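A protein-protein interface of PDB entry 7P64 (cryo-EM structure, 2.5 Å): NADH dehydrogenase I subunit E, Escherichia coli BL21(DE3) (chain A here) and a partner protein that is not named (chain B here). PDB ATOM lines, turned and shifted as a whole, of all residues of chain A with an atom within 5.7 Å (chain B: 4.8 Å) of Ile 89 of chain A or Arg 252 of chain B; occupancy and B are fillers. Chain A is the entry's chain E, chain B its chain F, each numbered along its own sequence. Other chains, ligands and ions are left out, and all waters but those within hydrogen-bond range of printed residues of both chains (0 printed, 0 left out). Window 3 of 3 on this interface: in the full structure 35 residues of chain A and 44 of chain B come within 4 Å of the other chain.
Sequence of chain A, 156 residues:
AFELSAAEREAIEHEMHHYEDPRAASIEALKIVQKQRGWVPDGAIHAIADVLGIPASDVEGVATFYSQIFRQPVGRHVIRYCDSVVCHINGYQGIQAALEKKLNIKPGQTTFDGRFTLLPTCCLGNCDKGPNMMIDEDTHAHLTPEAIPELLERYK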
ATOM      1  N   SER A  84     -16.419 -17.202  22.819  1.00  0.00           N
ATOM      2  CA  SER A  84     -15.432 -17.327  21.760  1.00  0.00           C
ATOM      3  C   SER A  84     -15.754 -16.354  20.627  1.00  0.00           C
ATOM      4  O   SER A  84     -16.647 -15.513  20.738  1.00  0.00           O
ATOM      5  CB  SER A  84     -15.353 -18.773  21.283  1.00  0.00           C
ATOM      6  OG  SER A  84     -14.694 -19.582  22.238  1.00  0.00           O
ATOM      7  N   VAL A  85     -15.027 -16.480  19.515  1.00  0.00           N
ATOM      8  CA  VAL A  85     -14.940 -15.399  18.536  1.00  0.00           C
ATOM      9  C   VAL A  85     -16.233 -15.262  17.730  1.00  0.00           C
ATOM     10  O   VAL A  85     -16.701 -14.145  17.478  1.00  0.00           O
ATOM     11  CB  VAL A  85     -13.699 -15.606  17.640  1.00  0.00           C
ATOM     12  CG1 VAL A  85     -13.650 -17.011  17.055  1.00  0.00           C
ATOM     13  CG2 VAL A  85     -13.615 -14.553  16.556  1.00  0.00           C
ATOM     14  N   VAL A  86     -16.840 -16.381  17.326  1.00  0.00           N
ATOM     15  CA  VAL A  86     -18.051 -16.306  16.515  1.00  0.00           C
ATOM     16  C   VAL A  86     -19.228 -15.817  17.349  1.00  0.00           C
ATOM     17  O   VAL A  86     -20.062 -15.039  16.872  1.00  0.00           O
ATOM     18  CB  VAL A  86     -18.345 -17.664  15.854  1.00  0.00           C
ATOM     19  CG1 VAL A  86     -19.352 -17.497  14.736  1.00  0.00           C
ATOM     20  CG2 VAL A  86     -17.067 -18.275  15.327  1.00  0.00           C
ATOM     21  N   CYS A  87     -19.317 -16.257  18.603  1.00  0.00           N
ATOM     22  CA  CYS A  87     -20.342 -15.727  19.490  1.00  0.00           C
ATOM     23  C   CYS A  87     -20.023 -14.311  19.949  1.00  0.00           C
ATOM     24  O   CYS A  87     -20.925 -13.606  20.412  1.00  0.00           O
ATOM     25  CB  CYS A  87     -20.526 -16.649  20.694  1.00  0.00           C
ATOM     26  SG  CYS A  87     -21.181 -18.275  20.271  1.00  0.00           S
ATOM     27  N   HIS A  88     -18.760 -13.885  19.846  1.00  0.00           N
ATOM     28  CA  HIS A  88     -18.436 -12.478  20.052  1.00  0.00           C
ATOM     29  C   HIS A  88     -18.951 -11.628  18.902  1.00  0.00           C
ATOM     30  O   HIS A  88     -19.460 -10.523  19.118  1.00  0.00           O
ATOM     31  CB  HIS A  88     -16.927 -12.302  20.220  1.00  0.00           C
ATOM     32  CG  HIS A  88     -16.488 -10.873  20.289  1.00  0.00           C
ATOM     33  ND1 HIS A  88     -16.463 -10.159  21.468  1.00  0.00           N
ATOM     34  CD2 HIS A  88     -16.053 -10.026  19.328  1.00  0.00           C
ATOM     35  CE1 HIS A  88     -16.035  -8.934  21.228  1.00  0.00           C
ATOM     36  NE2 HIS A  88     -15.780  -8.826  19.937  1.00  0.00           N
ATOM     37  N   ILE A  89     -18.812 -12.128  17.674  1.00  0.00           N
ATOM     38  CA  ILE A  89     -19.371 -11.439  16.516  1.00  0.00           C
ATOM     39  C   ILE A  89     -20.893 -11.421  16.594  1.00  0.00           C
ATOM     40  O   ILE A  89     -21.534 -10.413  16.278  1.00  0.00           O
ATOM     41  CB  ILE A  89     -18.858 -12.100  15.223  1.00  0.00           C
ATOM     42  CG1 ILE A  89     -17.355 -11.869  15.088  1.00  0.00           C
ATOM     43  CG2 ILE A  89     -19.569 -11.556  14.008  1.00  0.00           C
ATOM     44  CD1 ILE A  89     -16.763 -12.377  13.801  1.00  0.00           C
ATOM     45  N   ASN A  90     -21.492 -12.514  17.061  1.00  0.00           N
ATOM     46  CA  ASN A  90     -22.934 -12.580  17.254  1.00  0.00           C
ATOM     47  C   ASN A  90     -23.389 -11.936  18.558  1.00  0.00           C
ATOM     48  O   ASN A  90     -24.590 -11.942  18.846  1.00  0.00           O
ATOM     49  CB  ASN A  90     -23.405 -14.034  17.203  1.00  0.00           C
ATOM     50  CG  ASN A  90     -23.254 -14.642  15.828  1.00  0.00           C
ATOM     51  OD1 ASN A  90     -22.661 -15.708  15.668  1.00  0.00           O
ATOM     52  ND2 ASN A  90     -23.786 -13.963  14.822  1.00  0.00           N
ATOM     53  N   GLY A  91     -22.470 -11.388  19.347  1.00  0.00           N
ATOM     54  CA  GLY A  91     -22.836 -10.615  20.516  1.00  0.00           C
ATOM     55  C   GLY A  91     -23.200 -11.403  21.756  1.00  0.00           C
ATOM     56  O   GLY A  91     -24.344 -11.340  22.214  1.00  0.00           O
ATOM     57  N   SER B 250     -19.827 -18.525   8.575  1.00  0.00           N
ATOM     58  CA  SER B 250     -20.534 -18.235   9.813  1.00  0.00           C
ATOM     59  C   SER B 250     -20.230 -16.818  10.280  1.00  0.00           C
ATOM     60  O   SER B 250     -19.143 -16.286  10.047  1.00  0.00           O
ATOM     61  CB  SER B 250     -20.165 -19.231  10.917  1.00  0.00           C
ATOM     62  OG  SER B 250     -18.800 -19.118  11.272  1.00  0.00           O
ATOM     63  N   GLY B 251     -21.212 -16.218  10.946  1.00  0.00           N
ATOM     64  CA  GLY B 251     -21.041 -14.932  11.590  1.00  0.00           C
ATOM     65  C   GLY B 251     -21.637 -13.767  10.828  1.00  0.00           C
ATOM     66  O   GLY B 251     -20.999 -13.227   9.920  1.00  0.00           O
ATOM     67  N   ARG B 252     -22.853 -13.368  11.222  1.00  0.00           N
ATOM     68  CA  ARG B 252     -23.571 -12.217  10.659  1.00  0.00           C
ATOM     69  C   ARG B 252     -23.710 -12.304   9.140  1.00  0.00           C
ATOM     70  O   ARG B 252     -23.554 -11.316   8.420  1.00  0.00           O
ATOM     71  CB  ARG B 252     -22.914 -10.902  11.076  1.00  0.00           C
ATOM     72  CG  ARG B 252     -22.814 -10.741  12.576  1.00  0.00           C
ATOM     73  CD  ARG B 252     -23.714  -9.637  13.085  1.00  0.00           C
ATOM     74  NE  ARG B 252     -23.026  -8.353  13.086  1.00  0.00           N
ATOM     75  CZ  ARG B 252     -22.805  -7.625  14.171  1.00  0.00           C
ATOM     76  NH1 ARG B 252     -23.221  -8.018  15.363  1.00  0.00           N
ATOM     77  NH2 ARG B 252     -22.149  -6.474  14.057  1.00  0.00           N
ATOM     78  N   VAL B 253     -24.003 -13.502   8.650  1.00  0.00           N
ATOM     79  CA  VAL B 253     -24.334 -13.712   7.253  1.00  0.00           C
ATOM     80  C   VAL B 253     -25.814 -14.068   7.166  1.00  0.00           C
ATOM     81  O   VAL B 253     -26.477 -14.312   8.173  1.00  0.00           O
ATOM     82  CB  VAL B 253     -23.452 -14.793   6.601  1.00  0.00           C
ATOM     83  CG1 VAL B 253     -22.041 -14.278   6.426  1.00  0.00           C
ATOM     84  CG2 VAL B 253     -23.449 -16.047   7.442  1.00  0.00           C
ATOM     85  N   LYS B 254     -26.338 -14.073   5.938  1.00  0.00           N
ATOM     86  CA  LYS B 254     -27.762 -14.331   5.748  1.00  0.00           C
ATOM     87  C   LYS B 254     -28.119 -15.776   6.070  1.00  0.00           C
ATOM     88  O   LYS B 254     -29.151 -16.041   6.695  1.00  0.00           O
ATOM     89  CB  LYS B 254     -28.173 -13.982   4.318  1.00  0.00           C
ATOM     90  CG  LYS B 254     -28.417 -12.501   4.097  1.00  0.00           C
ATOM     91  CD  LYS B 254     -29.235 -12.256   2.845  1.00  0.00           C
ATOM     92  CE  LYS B 254     -29.333 -10.772   2.539  1.00  0.00           C
ATOM     93  NZ  LYS B 254     -30.147 -10.054   3.557  1.00  0.00           N
ATOM     94  N   MET B 278     -23.568 -10.997   3.194  1.00  0.00           N
ATOM     95  CA  MET B 278     -23.691 -10.386   4.505  1.00  0.00           C
ATOM     96  C   MET B 278     -25.146 -10.018   4.785  1.00  0.00           C
ATOM     97  O   MET B 278     -26.014 -10.085   3.912  1.00  0.00           O
ATOM     98  CB  MET B 278     -22.797  -9.154   4.606  1.00  0.00           C
ATOM     99  CG  MET B 278     -21.321  -9.449   4.413  1.00  0.00           C
ATOM    100  SD  MET B 278     -20.687 -10.634   5.614  1.00  0.00           S
ATOM    101  CE  MET B 278     -20.628  -9.625   7.089  1.00  0.00           C
ATOM    102  N   ARG B 279     -25.407  -9.624   6.027  1.00  0.00           N
ATOM    103  CA  ARG B 279     -26.750  -9.246   6.432  1.00  0.00           C
ATOM    104  C   ARG B 279     -27.057  -7.820   5.981  1.00  0.00           C
ATOM    105  O   ARG B 279     -26.258  -7.162   5.309  1.00  0.00           O
ATOM    106  CB  ARG B 279     -26.910  -9.392   7.943  1.00  0.00           C
ATOM    107  CG  ARG B 279     -26.985 -10.830   8.414  1.00  0.00           C
ATOM    108  CD  ARG B 279     -28.069 -11.009   9.460  1.00  0.00           C
ATOM    109  NE  ARG B 279     -27.828 -10.185  10.638  1.00  0.00           N
ATOM    110  CZ  ARG B 279     -27.298 -10.633  11.767  1.00  0.00           C
ATOM    111  NH1 ARG B 279     -26.939 -11.898  11.907  1.00  0.00           N
ATOM    112  NH2 ARG B 279     -27.126  -9.790  12.782  1.00  0.00           N
ATOM    113  N   LEU B 282     -24.762  -4.311   6.828  1.00  0.00           N
ATOM    114  CA  LEU B 282     -23.410  -4.684   7.220  1.00  0.00           C
ATOM    115  C   LEU B 282     -22.597  -4.981   5.971  1.00  0.00           C
ATOM    116  O   LEU B 282     -23.050  -5.723   5.094  1.00  0.00           O
ATOM    117  CB  LEU B 282     -23.419  -5.902   8.144  1.00  0.00           C
ATOM    118  CG  LEU B 282     -24.287  -5.798   9.398  1.00  0.00           C
ATOM    119  CD1 LEU B 282     -24.331  -7.130  10.124  1.00  0.00           C
ATOM    120  CD2 LEU B 282     -23.771  -4.701  10.313  1.00  0.00           C
ATOM    121  N   MET B 324     -15.246 -17.755   8.735  1.00  0.00           N
ATOM    122  CA  MET B 324     -15.983 -16.838   9.591  1.00  0.00           C
ATOM    123  C   MET B 324     -15.836 -15.430   9.040  1.00  0.00           C
ATOM    124  O   MET B 324     -14.724 -15.003   8.715  1.00  0.00           O
ATOM    125  CB  MET B 324     -15.480 -16.909  11.033  1.00  0.00           C
ATOM    126  CG  MET B 324     -16.144 -15.926  11.973  1.00  0.00           C
ATOM    127  SD  MET B 324     -15.165 -15.663  13.457  1.00  0.00           S
ATOM    128  CE  MET B 324     -13.829 -14.668  12.809  1.00  0.00           C
ATOM    129  N   ALA B 325     -16.953 -14.718   8.938  1.00  0.00           N
ATOM    130  CA  ALA B 325     -16.994 -13.396   8.328  1.00  0.00           C
ATOM    131  C   ALA B 325     -17.061 -12.319   9.402  1.00  0.00           C
ATOM    132  O   ALA B 325     -17.866 -12.411  10.333  1.00  0.00           O
ATOM    133  CB  ALA B 325     -18.190 -13.271   7.384  1.00  0.00           C
ATOM    134  N   VAL B 326     -16.219 -11.299   9.261  1.00  0.00           N
ATOM    135  CA  VAL B 326     -16.160 -10.157  10.163  1.00  0.00           C
ATOM    136  C   VAL B 326     -16.598  -8.930   9.382  1.00  0.00           C
ATOM    137  O   VAL B 326     -16.017  -8.619   8.334  1.00  0.00           O
ATOM    138  CB  VAL B 326     -14.742  -9.957  10.728  1.00  0.00           C
ATOM    139  CG1 VAL B 326     -14.749  -8.919  11.830  1.00  0.00           C
ATOM    140  CG2 VAL B 326     -14.173 -11.273  11.225  1.00  0.00           C
ATOM    141  N   ASP B 327     -17.607  -8.232   9.895  1.00  0.00           N
ATOM    142  CA  ASP B 327     -18.168  -7.062   9.239  1.00  0.00           C
ATOM    143  C   ASP B 327     -17.440  -5.799   9.699  1.00  0.00           C
ATOM    144  O   ASP B 327     -16.457  -5.854  10.441  1.00  0.00           O
ATOM    145  CB  ASP B 327     -19.667  -6.974   9.511  1.00  0.00           C
ATOM    146  CG  ASP B 327     -20.010  -7.228  10.962  1.00  0.00           C
ATOM    147  OD1 ASP B 327     -19.252  -7.959  11.630  1.00  0.00           O
ATOM    148  OD2 ASP B 327     -21.032  -6.694  11.437  1.00  0.00           O
ATOM    149  N   GLU B 329     -18.651  -3.440  11.619  1.00  0.00           N
ATOM    150  CA  GLU B 329     -19.017  -3.018  12.967  1.00  0.00           C
ATOM    151  C   GLU B 329     -18.044  -3.556  14.011  1.00  0.00           C
ATOM    152  O   GLU B 329     -17.777  -2.885  15.014  1.00  0.00           O
ATOM    153  CB  GLU B 329     -20.447  -3.468  13.275  1.00  0.00           C
ATOM    154  CG  GLU B 329     -20.964  -3.075  14.651  1.00  0.00           C
ATOM    155  CD  GLU B 329     -22.442  -3.359  14.822  1.00  0.00           C
ATOM    156  OE1 GLU B 329     -23.190  -3.242  13.828  1.00  0.00           O
ATOM    157  OE2 GLU B 329     -22.857  -3.705  15.948  1.00  0.00           O
ATOM    158  N   ILE B 330     -17.491  -4.742  13.784  1.00  0.00           N
ATOM    159  CA  ILE B 330     -16.627  -5.393  14.762  1.00  0.00           C
ATOM    160  C   ILE B 330     -15.269  -4.704  14.773  1.00  0.00           C
ATOM    161  O   ILE B 330     -14.621  -4.568  13.730  1.00  0.00           O
ATOM    162  CB  ILE B 330     -16.483  -6.891  14.456  1.00  0.00           C
ATOM    163  CG1 ILE B 330     -17.832  -7.599  14.586  1.00  0.00           C
ATOM    164  CG2 ILE B 330     -15.453  -7.529  15.372  1.00  0.00           C
ATOM    165  CD1 ILE B 330     -18.459  -7.475  15.950  1.00  0.00           C
ATOM    166  N   LEU B 335     -11.719  -8.059  18.692  1.00  0.00           N
ATOM    167  CA  LEU B 335     -11.819  -9.417  18.169  1.00  0.00           C
ATOM    168  C   LEU B 335     -10.535 -10.200  18.410  1.00  0.00           C
ATOM    169  O   LEU B 335     -10.567 -11.357  18.850  1.00  0.00           O
ATOM    170  CB  LEU B 335     -12.142  -9.366  16.678  1.00  0.00           C
ATOM    171  CG  LEU B 335     -12.656 -10.651  16.045  1.00  0.00           C
ATOM    172  CD1 LEU B 335     -14.085 -10.879  16.467  1.00  0.00           C
ATOM    173  CD2 LEU B 335     -12.549 -10.558  14.541  1.00  0.00           C
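NH1 of Arg 252 of chain B lies within hydrogen-bond range of O of Ile 89 of chain A (3.1 Å).
N of Ala 325 of chain B sits at hydrogen-bond distance from O of Ser 250 of chain B, 2.9 Å away.
The backbone carbonyl oxygen of Arg 252 of chain B lies close to the backbone NH of Arg 279 of chain B, at 3.5 Å.
The guanidinium group of Arg 252 of chain B lies within salt-bridge range of the side-chain carboxylate of Asp 327 of chain B.
NH2 of Arg 252 of chain B is in salt-bridge range of OE1 of Glu 329 of chain B (3.4 Å).
The backbone carbonyl oxygen of Val 86 of chain A lies close to the side-chain amide oxygen of Asn 90 of chain A, at 2.9 Å.
SD of Met 324 of chain B touches CG2 of Val 85 of chain A, 3.6 Å away.
CG2 of Val 85 of chain A touches CD1 of Leu 335 of chain B (3.7 Å).
Val 86 of chain A touches Ser 250 of chain B (CG1 to OG, 3.9 Å).
SD of Met 324 of chain B touches CG2 of Val 86 of chain A (3.7 Å).
CD1 of Leu 335 of chain B touches CD2 of His 88 of chain A, 3.6 Å away.
Ile 89 of chain A touches Met 324 of chain B (CD1 to SD, 3.7 Å).
Ala 325 of chain B touches Ile 89 of chain A.
Val 326 of chain B touches Ile 89 of chain A (CG2 to CD1, 3.8 Å).
CD1 of Leu 335 of chain B touches CG1 of Ile 89 of chain A, 3.7 Å away.
ND2 of Asn 90 of chain A touches N of Arg 252 of chain B (3.8 Å).
Arg 252 of chain B touches just these residues of chain A: Ile 89 and Asn 90.
Of the printed residues of chain A, Met 324 of chain B touches Val 85 (3.6 Å), Val 86 (3.7 Å) and Ile 89 (3.7 Å).
Glu 329 of chain B touches none of the printed residues of chain A.
Of the printed residues of chain A, Leu 335 of chain B touches Val 85, His 88 and Ile 89.
The nearest residue of chain A that does not touch Arg 252 of chain B is Gly 91 of chain A (5.3 Å).
Hydrophobic or aromatic side chains of chain B within 4 Å of the printed part of chain A: Met 324, Val 326 and Leu 335.
Printed residues of chain A that touch a printed residue of chain B: Val 85, Val 86, His 88, Ile 89 and Asn 90.
Among the printed residues, no Asp or Glu carboxylate lies within 4 Å of a Lys or Arg side-chain nitrogen of the other chain.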
